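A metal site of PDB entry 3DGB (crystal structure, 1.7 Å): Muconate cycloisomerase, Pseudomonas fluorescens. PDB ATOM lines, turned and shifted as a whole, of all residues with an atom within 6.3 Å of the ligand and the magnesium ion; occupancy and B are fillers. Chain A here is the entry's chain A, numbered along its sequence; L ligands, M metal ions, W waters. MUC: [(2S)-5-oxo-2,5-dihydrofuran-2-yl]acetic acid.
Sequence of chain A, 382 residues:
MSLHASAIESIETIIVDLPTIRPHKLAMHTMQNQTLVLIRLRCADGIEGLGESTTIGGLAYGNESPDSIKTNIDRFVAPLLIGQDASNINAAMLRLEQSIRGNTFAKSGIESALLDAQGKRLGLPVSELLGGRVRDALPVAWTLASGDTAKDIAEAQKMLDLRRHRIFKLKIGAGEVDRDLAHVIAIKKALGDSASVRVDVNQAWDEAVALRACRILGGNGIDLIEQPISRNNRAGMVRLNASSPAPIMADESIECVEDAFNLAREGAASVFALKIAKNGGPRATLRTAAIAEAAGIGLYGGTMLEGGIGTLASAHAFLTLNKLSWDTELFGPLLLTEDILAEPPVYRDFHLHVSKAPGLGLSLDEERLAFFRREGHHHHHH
Tyr 61 touches the magnesium ion (OH to MG, 3.9 Å).
NZ of Lys 169 touches the magnesium ion, 3.98 Å away.
Asn 202 touches the magnesium ion (ND2 to MG, 3.5 Å).
OE1 of Glu 252 touches the magnesium ion, 3.7 Å away.
Within 4 Å of the magnesium ion: Tyr 61, Lys 169, Asp 200, Asn 202, Glu 226, Asp 251 and Glu 252.
Water W1 lies within hydrogen-bond range of the side-chain carboxylate (OE1) of Glu 252 (2.5 Å), the side-chain carboxylate (OD1) of Asp 200 (2.6 Å) and the side-chain amide nitrogen (ND2) of Asn 202 (3.3 Å).
The side-chain amino group (NZ) of Lys 171 is in salt-bridge range of an oxygen (O2) of the ligand, 2.5 Å away.
An oxygen (O1) of the ligand lies close to the side-chain hydroxyl (OH) of Tyr 61 (2.6 Å).
The side-chain amino group (NZ) of Lys 169 lies within salt-bridge range of an oxygen (O2) of the ligand (2.8 Å).
NE2 of His 24 lies within hydrogen-bond range of O6 of the ligand (3.0 Å).
The side-chain amide nitrogen of Asn 202 lies close to an oxygen (O1) of the ligand (3.1 Å).
OG1 of Thr 143 lies within hydrogen-bond range of O6 of the ligand (3.2 Å).
NZ of Lys 275 lies close to O1 of the ligand (3.4 Å).
OD1 of Asp 251 lies within salt-bridge range of NZ of Lys 275 (3.1 Å).
The side-chain carboxylate of Glu 226 lies within salt-bridge range of the side-chain amino group of Lys 169.
The side-chain amino group of Lys 171 sits at hydrogen-bond distance from the side-chain amide oxygen of Asn 202.
The backbone carbonyl oxygen (O) of His 24 sits at hydrogen-bond distance from the backbone NH (N) of Met 31, at 2.7 Å.
OE2 of Glu 252 lies within hydrogen-bond range of ND2 of Asn 202.
The backbone NH (N) of Thr 303 is in hydrogen-bond range of the side-chain carboxylate (OE2) of Glu 329 (2.9 Å).
The side-chain hydroxyl (OH) of Tyr 300 sits at hydrogen-bond distance from the side-chain carboxylate (OE1) of Glu 329 (2.7 Å).
The side-chain hydroxyl (OG1) of Thr 303 lies within hydrogen-bond range of the backbone NH (N) of Leu 305 (3.0 Å).
Ile 56 touches the ligand (CD1 to C2, 3.6 Å).
Thr 303 touches the ligand.
Leu 305 touches the ligand (CD2 to C6, 3.9 Å).
OE2 of Glu 329 touches C4 of the ligand (3.2 Å).
Phe 331 touches the ligand (CZ to O6, 3.6 Å).
Hydrophobic or aromatic side chains that line the ligand: His 24, Ile 56, Tyr 61, Leu 305 and Phe 331.
Of the 24 residues printed, 14 come within 4 Å of the ligand.
The nearest printed residue that does not touch the ligand is Glu 226 (4.1 Å).
The magnesium ion is bound by water W1 (1.8 Å), the side-chain carboxylate of Asp 251 (2.2 Å), the side-chain carboxylate of Glu 226 (2.3 Å), the side-chain carboxylate of Asp 200 (2.3 Å) and an oxygen (O1) of the ligand (2.4 Å).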
ATOM      1  N   HIS A  24      27.230  -1.830  32.445  1.00  0.00           N
ATOM      2  CA  HIS A  24      26.684  -2.972  31.719  1.00  0.00           C
ATOM      3  C   HIS A  24      27.840  -3.559  30.909  1.00  0.00           C
ATOM      4  O   HIS A  24      28.248  -2.997  29.891  1.00  0.00           O
ATOM      5  CB  HIS A  24      25.570  -2.506  30.786  1.00  0.00           C
ATOM      6  CG  HIS A  24      24.612  -3.583  30.389  1.00  0.00           C
ATOM      7  ND1 HIS A  24      23.824  -4.263  31.298  1.00  0.00           N
ATOM      8  CD2 HIS A  24      24.281  -4.078  29.174  1.00  0.00           C
ATOM      9  CE1 HIS A  24      23.052  -5.127  30.665  1.00  0.00           C
ATOM     10  NE2 HIS A  24      23.313  -5.032  29.366  1.00  0.00           N
ATOM     11  N   LEU A  26      29.532  -6.065  28.412  1.00  0.00           N
ATOM     12  CA  LEU A  26      29.345  -6.990  27.293  1.00  0.00           C
ATOM     13  C   LEU A  26      30.730  -7.542  26.974  1.00  0.00           C
ATOM     14  O   LEU A  26      31.743  -7.022  27.446  1.00  0.00           O
ATOM     15  CB  LEU A  26      28.779  -6.272  26.067  1.00  0.00           C
ATOM     16  CG  LEU A  26      27.478  -5.463  26.213  1.00  0.00           C
ATOM     17  CD1 LEU A  26      26.846  -5.323  24.831  1.00  0.00           C
ATOM     18  CD2 LEU A  26      26.512  -6.159  27.151  1.00  0.00           C
ATOM     19  N   MET A  28      32.573  -7.325  24.390  1.00  0.00           N
ATOM     20  CA  MET A  28      33.463  -6.379  23.702  1.00  0.00           C
ATOM     21  C   MET A  28      33.485  -4.965  24.265  1.00  0.00           C
ATOM     22  O   MET A  28      34.374  -4.180  23.928  1.00  0.00           O
ATOM     23  CB  MET A  28      33.073  -6.297  22.221  1.00  0.00           C
ATOM     24  CG  MET A  28      31.980  -5.259  21.886  1.00  0.00           C
ATOM     25  SD  MET A  28      30.377  -5.497  22.708  1.00  0.00           S
ATOM     26  CE  MET A  28      29.730  -6.871  21.739  1.00  0.00           C
ATOM     27  N   MET A  31      29.452  -0.674  29.125  1.00  0.00           N
ATOM     28  CA  MET A  31      28.656   0.537  29.088  1.00  0.00           C
ATOM     29  C   MET A  31      28.680   1.272  30.429  1.00  0.00           C
ATOM     30  O   MET A  31      28.489   0.649  31.480  1.00  0.00           O
ATOM     31  CB  MET A  31      27.197   0.203  28.740  1.00  0.00           C
ATOM     32  CG  MET A  31      26.992  -0.351  27.344  1.00  0.00           C
ATOM     33  SD  MET A  31      25.270  -0.848  27.082  1.00  0.00           S
ATOM     34  CE  MET A  31      24.485   0.761  26.970  1.00  0.00           C
ATOM     35  N   ILE A  56      25.089   0.624  20.740  1.00  0.00           N
ATOM     36  CA  ILE A  56      25.841   0.349  21.952  1.00  0.00           C
ATOM     37  C   ILE A  56      27.343   0.598  21.783  1.00  0.00           C
ATOM     38  O   ILE A  56      27.950   0.135  20.825  1.00  0.00           O
ATOM     39  CB  ILE A  56      25.638  -1.125  22.407  1.00  0.00           C
ATOM     40  CG1 ILE A  56      24.179  -1.353  22.798  1.00  0.00           C
ATOM     41  CG2 ILE A  56      26.576  -1.451  23.563  1.00  0.00           C
ATOM     42  CD1 ILE A  56      23.839  -2.801  23.106  1.00  0.00           C
ATOM     43  N   TYR A  61      29.961  -1.952  18.802  1.00  0.00           N
ATOM     44  CA  TYR A  61      28.967  -2.970  18.472  1.00  0.00           C
ATOM     45  C   TYR A  61      28.700  -3.047  16.970  1.00  0.00           C
ATOM     46  O   TYR A  61      28.843  -4.110  16.360  1.00  0.00           O
ATOM     47  CB  TYR A  61      27.659  -2.692  19.216  1.00  0.00           C
ATOM     48  CG  TYR A  61      26.699  -3.857  19.200  1.00  0.00           C
ATOM     49  CD1 TYR A  61      26.604  -4.729  20.280  1.00  0.00           C
ATOM     50  CD2 TYR A  61      25.899  -4.100  18.084  1.00  0.00           C
ATOM     51  CE1 TYR A  61      25.741  -5.818  20.251  1.00  0.00           C
ATOM     52  CE2 TYR A  61      25.035  -5.187  18.046  1.00  0.00           C
ATOM     53  CZ  TYR A  61      24.957  -6.032  19.133  1.00  0.00           C
ATOM     54  OH  TYR A  61      24.095  -7.103  19.088  1.00  0.00           O
ATOM     55  N   THR A 143      18.884  -8.544  31.619  1.00  0.00           N
ATOM     56  CA  THR A 143      20.269  -8.955  31.439  1.00  0.00           C
ATOM     57  C   THR A 143      21.106  -8.726  32.685  1.00  0.00           C
ATOM     58  O   THR A 143      21.063  -7.656  33.296  1.00  0.00           O
ATOM     59  CB  THR A 143      20.926  -8.211  30.259  1.00  0.00           C
ATOM     60  OG1 THR A 143      20.270  -8.587  29.046  1.00  0.00           O
ATOM     61  CG2 THR A 143      22.403  -8.550  30.168  1.00  0.00           C
ATOM     62  N   LYS A 169      19.165 -13.040  31.038  1.00  0.00           N
ATOM     63  CA  LYS A 169      20.155 -13.162  29.975  1.00  0.00           C
ATOM     64  C   LYS A 169      21.516 -12.799  30.558  1.00  0.00           C
ATOM     65  O   LYS A 169      21.684 -11.715  31.109  1.00  0.00           O
ATOM     66  CB  LYS A 169      19.784 -12.225  28.834  1.00  0.00           C
ATOM     67  CG  LYS A 169      20.870 -11.996  27.797  1.00  0.00           C
ATOM     68  CD  LYS A 169      20.303 -11.224  26.616  1.00  0.00           C
ATOM     69  CE  LYS A 169      21.393 -10.686  25.720  1.00  0.00           C
ATOM     70  NZ  LYS A 169      20.839 -10.176  24.441  1.00  0.00           N
ATOM     71  N   LYS A 171      25.509 -12.068  30.042  1.00  0.00           N
ATOM     72  CA  LYS A 171      26.546 -11.664  29.112  1.00  0.00           C
ATOM     73  C   LYS A 171      27.856 -12.352  29.471  1.00  0.00           C
ATOM     74  O   LYS A 171      28.350 -12.217  30.583  1.00  0.00           O
ATOM     75  CB  LYS A 171      26.767 -10.152  29.193  1.00  0.00           C
ATOM     76  CG  LYS A 171      25.632  -9.328  28.649  1.00  0.00           C
ATOM     77  CD  LYS A 171      25.472  -9.604  27.178  1.00  0.00           C
ATOM     78  CE  LYS A 171      24.462  -8.689  26.553  1.00  0.00           C
ATOM     79  NZ  LYS A 171      24.538  -8.836  25.082  1.00  0.00           N
ATOM     80  N   ASP A 200      24.470 -14.877  26.238  1.00  0.00           N
ATOM     81  CA  ASP A 200      24.761 -14.168  24.991  1.00  0.00           C
ATOM     82  C   ASP A 200      26.276 -14.010  25.005  1.00  0.00           C
ATOM     83  O   ASP A 200      26.826 -13.390  25.919  1.00  0.00           O
ATOM     84  CB  ASP A 200      24.105 -12.783  24.976  1.00  0.00           C
ATOM     85  CG  ASP A 200      24.280 -12.072  23.638  1.00  0.00           C
ATOM     86  OD1 ASP A 200      25.067 -12.556  22.795  1.00  0.00           O
ATOM     87  OD2 ASP A 200      23.639 -11.019  23.426  1.00  0.00           O
ATOM     88  N   ASN A 202      27.945 -12.705  22.367  1.00  0.00           N
ATOM     89  CA  ASN A 202      28.286 -11.619  21.462  1.00  0.00           C
ATOM     90  C   ASN A 202      29.435 -11.940  20.503  1.00  0.00           C
ATOM     91  O   ASN A 202      30.379 -11.155  20.351  1.00  0.00           O
ATOM     92  CB  ASN A 202      28.616 -10.345  22.255  1.00  0.00           C
ATOM     93  CG  ASN A 202      27.381  -9.700  22.885  1.00  0.00           C
ATOM     94  OD1 ASN A 202      27.218  -9.688  24.106  1.00  0.00           O
ATOM     95  ND2 ASN A 202      26.493  -9.177  22.036  1.00  0.00           N
ATOM     96  N   GLU A 226      22.856 -17.417  22.735  1.00  0.00           N
ATOM     97  CA  GLU A 226      22.837 -16.364  21.723  1.00  0.00           C
ATOM     98  C   GLU A 226      24.203 -16.053  21.117  1.00  0.00           C
ATOM     99  O   GLU A 226      25.175 -15.828  21.844  1.00  0.00           O
ATOM    100  CB  GLU A 226      22.240 -15.089  22.329  1.00  0.00           C
ATOM    101  CG  GLU A 226      22.000 -13.968  21.346  1.00  0.00           C
ATOM    102  CD  GLU A 226      21.395 -12.728  22.006  1.00  0.00           C
ATOM    103  OE1 GLU A 226      20.952 -12.840  23.169  1.00  0.00           O
ATOM    104  OE2 GLU A 226      21.367 -11.658  21.369  1.00  0.00           O
ATOM    105  N   GLN A 227      24.243 -16.063  19.783  1.00  0.00           N
ATOM    106  CA  GLN A 227      25.425 -15.766  18.969  1.00  0.00           C
ATOM    107  C   GLN A 227      26.756 -16.156  19.620  1.00  0.00           C
ATOM    108  O   GLN A 227      27.570 -15.303  19.961  1.00  0.00           O
ATOM    109  CB  GLN A 227      25.434 -14.273  18.614  1.00  0.00           C
ATOM    110  CG  GLN A 227      26.308 -13.866  17.429  1.00  0.00           C
ATOM    111  CD  GLN A 227      25.719 -14.256  16.078  1.00  0.00           C
ATOM    112  OE1 GLN A 227      24.526 -14.082  15.835  1.00  0.00           O
ATOM    113  NE2 GLN A 227      26.573 -14.763  15.188  1.00  0.00           N
ATOM    114  N   ASP A 251      21.879 -13.271  16.294  1.00  0.00           N
ATOM    115  CA  ASP A 251      21.630 -11.859  16.571  1.00  0.00           C
ATOM    116  C   ASP A 251      22.482 -11.054  15.610  1.00  0.00           C
ATOM    117  O   ASP A 251      21.983 -10.576  14.591  1.00  0.00           O
ATOM    118  CB  ASP A 251      21.965 -11.506  18.028  1.00  0.00           C
ATOM    119  CG  ASP A 251      21.807 -10.016  18.314  1.00  0.00           C
ATOM    120  OD1 ASP A 251      21.123  -9.338  17.512  1.00  0.00           O
ATOM    121  OD2 ASP A 251      22.338  -9.523  19.330  1.00  0.00           O
ATOM    122  N   GLU A 252      23.763 -10.906  15.913  1.00  0.00           N
ATOM    123  CA  GLU A 252      24.656 -10.156  15.041  1.00  0.00           C
ATOM    124  C   GLU A 252      24.697 -10.731  13.627  1.00  0.00           C
ATOM    125  O   GLU A 252      25.011 -10.010  12.671  1.00  0.00           O
ATOM    126  CB  GLU A 252      26.072 -10.116  15.645  1.00  0.00           C
ATOM    127  CG  GLU A 252      26.183  -9.220  16.871  1.00  0.00           C
ATOM    128  CD  GLU A 252      26.069  -9.967  18.189  1.00  0.00           C
ATOM    129  OE1 GLU A 252      25.280 -10.934  18.262  1.00  0.00           O
ATOM    130  OE2 GLU A 252      26.747  -9.575  19.158  1.00  0.00           O
ATOM    131  N   LYS A 275      15.418  -7.271  15.803  1.00  0.00           N
ATOM    132  CA  LYS A 275      15.793  -5.928  16.221  1.00  0.00           C
ATOM    133  C   LYS A 275      15.477  -4.927  15.126  1.00  0.00           C
ATOM    134  O   LYS A 275      15.947  -5.058  13.995  1.00  0.00           O
ATOM    135  CB  LYS A 275      17.281  -5.884  16.578  1.00  0.00           C
ATOM    136  CG  LYS A 275      17.634  -6.776  17.752  1.00  0.00           C
ATOM    137  CD  LYS A 275      19.107  -6.660  18.148  1.00  0.00           C
ATOM    138  CE  LYS A 275      19.394  -7.517  19.372  1.00  0.00           C
ATOM    139  NZ  LYS A 275      20.793  -7.364  19.850  1.00  0.00           N
ATOM    140  N   TYR A 300      12.345 -13.979  18.927  1.00  0.00           N
ATOM    141  CA  TYR A 300      12.759 -13.304  20.155  1.00  0.00           C
ATOM    142  C   TYR A 300      12.699 -11.812  19.883  1.00  0.00           C
ATOM    143  O   TYR A 300      13.236 -11.343  18.872  1.00  0.00           O
ATOM    144  CB  TYR A 300      14.194 -13.711  20.492  1.00  0.00           C
ATOM    145  CG  TYR A 300      14.784 -13.057  21.723  1.00  0.00           C
ATOM    146  CD1 TYR A 300      14.321 -13.393  22.994  1.00  0.00           C
ATOM    147  CD2 TYR A 300      15.876 -12.205  21.608  1.00  0.00           C
ATOM    148  CE1 TYR A 300      14.948 -12.901  24.133  1.00  0.00           C
ATOM    149  CE2 TYR A 300      16.509 -11.707  22.748  1.00  0.00           C
ATOM    150  CZ  TYR A 300      16.052 -12.061  24.004  1.00  0.00           C
ATOM    151  OH  TYR A 300      16.708 -11.634  25.126  1.00  0.00           O
ATOM    152  N   GLY A 302      14.136  -8.615  20.222  1.00  0.00           N
ATOM    153  CA  GLY A 302      15.401  -8.036  20.644  1.00  0.00           C
ATOM    154  C   GLY A 302      15.454  -6.533  20.817  1.00  0.00           C
ATOM    155  O   GLY A 302      14.522  -5.805  20.443  1.00  0.00           O
ATOM    156  N   THR A 303      16.565  -6.069  21.366  1.00  0.00           N
ATOM    157  CA  THR A 303      16.762  -4.642  21.590  1.00  0.00           C
ATOM    158  C   THR A 303      18.224  -4.254  21.436  1.00  0.00           C
ATOM    159  O   THR A 303      19.126  -5.106  21.552  1.00  0.00           O
ATOM    160  CB  THR A 303      16.306  -4.238  23.028  1.00  0.00           C
ATOM    161  OG1 THR A 303      16.352  -2.815  23.170  1.00  0.00           O
ATOM    162  CG2 THR A 303      17.213  -4.864  24.077  1.00  0.00           C
ATOM    163  N   MET A 304      18.468  -2.979  21.147  1.00  0.00           N
ATOM    164  CA  MET A 304      19.828  -2.454  21.059  1.00  0.00           C
ATOM    165  C   MET A 304      19.950  -1.479  22.232  1.00  0.00           C
ATOM    166  O   MET A 304      20.759  -0.549  22.212  1.00  0.00           O
ATOM    167  CB  MET A 304      20.075  -1.737  19.732  1.00  0.00           C
ATOM    168  CG  MET A 304      20.374  -2.674  18.543  1.00  0.00           C
ATOM    169  SD  MET A 304      21.777  -3.803  18.769  1.00  0.00           S
ATOM    170  CE  MET A 304      23.086  -2.624  19.291  1.00  0.00           C
ATOM    171  N   LEU A 305      19.125  -1.717  23.254  1.00  0.00           N
ATOM    172  CA  LEU A 305      19.074  -0.908  24.469  1.00  0.00           C
ATOM    173  C   LEU A 305      18.534   0.502  24.233  1.00  0.00           C
ATOM    174  O   LEU A 305      19.050   1.493  24.756  1.00  0.00           O
ATOM    175  CB  LEU A 305      20.450  -0.856  25.149  1.00  0.00           C
ATOM    176  CG  LEU A 305      20.944  -2.224  25.644  1.00  0.00           C
ATOM    177  CD1 LEU A 305      22.285  -2.073  26.349  1.00  0.00           C
ATOM    178  CD2 LEU A 305      19.914  -2.831  26.595  1.00  0.00           C
ATOM    179  N   GLU A 329      13.383  -8.911  25.199  1.00  0.00           N
ATOM    180  CA  GLU A 329      14.352  -8.279  26.081  1.00  0.00           C
ATOM    181  C   GLU A 329      14.157  -6.767  26.001  1.00  0.00           C
ATOM    182  O   GLU A 329      15.125  -6.000  25.999  1.00  0.00           O
ATOM    183  CB  GLU A 329      15.783  -8.644  25.674  1.00  0.00           C
ATOM    184  CG  GLU A 329      16.072  -8.475  24.188  1.00  0.00           C
ATOM    185  CD  GLU A 329      17.536  -8.703  23.836  1.00  0.00           C
ATOM    186  OE1 GLU A 329      18.202  -9.496  24.547  1.00  0.00           O
ATOM    187  OE2 GLU A 329      18.017  -8.111  22.847  1.00  0.00           O
ATOM    188  N   PHE A 331      13.874  -4.192  27.768  1.00  0.00           N
ATOM    189  CA  PHE A 331      14.096  -3.571  29.067  1.00  0.00           C
ATOM    190  C   PHE A 331      14.961  -2.322  29.013  1.00  0.00           C
ATOM    191  O   PHE A 331      15.347  -1.771  30.045  1.00  0.00           O
ATOM    192  CB  PHE A 331      14.732  -4.591  30.020  1.00  0.00           C
ATOM    193  CG  PHE A 331      16.124  -5.009  29.632  1.00  0.00           C
ATOM    194  CD1 PHE A 331      17.224  -4.203  29.927  1.00  0.00           C
ATOM    195  CD2 PHE A 331      16.341  -6.206  28.946  1.00  0.00           C
ATOM    196  CE1 PHE A 331      18.513  -4.580  29.551  1.00  0.00           C
ATOM    197  CE2 PHE A 331      17.623  -6.589  28.568  1.00  0.00           C
ATOM    198  CZ  PHE A 331      18.716  -5.778  28.875  1.00  0.00           C
ATOM    199  N   LEU A 335      17.095   0.223  32.078  1.00  0.00           N
ATOM    200  CA  LEU A 335      18.540   0.305  32.301  1.00  0.00           C
ATOM    201  C   LEU A 335      18.950   1.774  32.410  1.00  0.00           C
ATOM    202  O   LEU A 335      19.961   2.104  33.029  1.00  0.00           O
ATOM    203  CB  LEU A 335      19.290  -0.377  31.151  1.00  0.00           C
ATOM    204  CG  LEU A 335      20.817  -0.474  31.245  1.00  0.00           C
ATOM    205  CD1 LEU A 335      21.229  -1.261  32.475  1.00  0.00           C
ATOM    206  CD2 LEU A 335      21.345  -1.145  29.976  1.00  0.00           C
HETATM  207  C1  MUC L   1      22.972  -7.599  22.533  1.00  0.00           C
HETATM  208  O1  MUC L   1      23.661  -7.900  21.542  1.00  0.00           O
HETATM  209  O2  MUC L   1      22.675  -8.367  23.466  1.00  0.00           O
HETATM  210  C4  MUC L   1      20.429  -6.606  24.212  1.00  0.00           C
HETATM  211  C5  MUC L   1      20.360  -6.607  25.543  1.00  0.00           C
HETATM  212  C6  MUC L   1      21.569  -6.340  26.032  1.00  0.00           C
HETATM  213  O6  MUC L   1      21.874  -6.501  27.215  1.00  0.00           O
HETATM  214  O3  MUC L   1      22.460  -5.885  25.085  1.00  0.00           O
HETATM  215  C3  MUC L   1      21.657  -5.745  23.902  1.00  0.00           C
HETATM  216  C2  MUC L   1      22.452  -6.131  22.610  1.00  0.00           C
HETATM  217 MG    MG M   1      23.227 -10.259  21.260  1.00  0.00          MG
HETATM  218  O   HOH W   1      24.479 -11.361  20.607  1.00  0.00           O
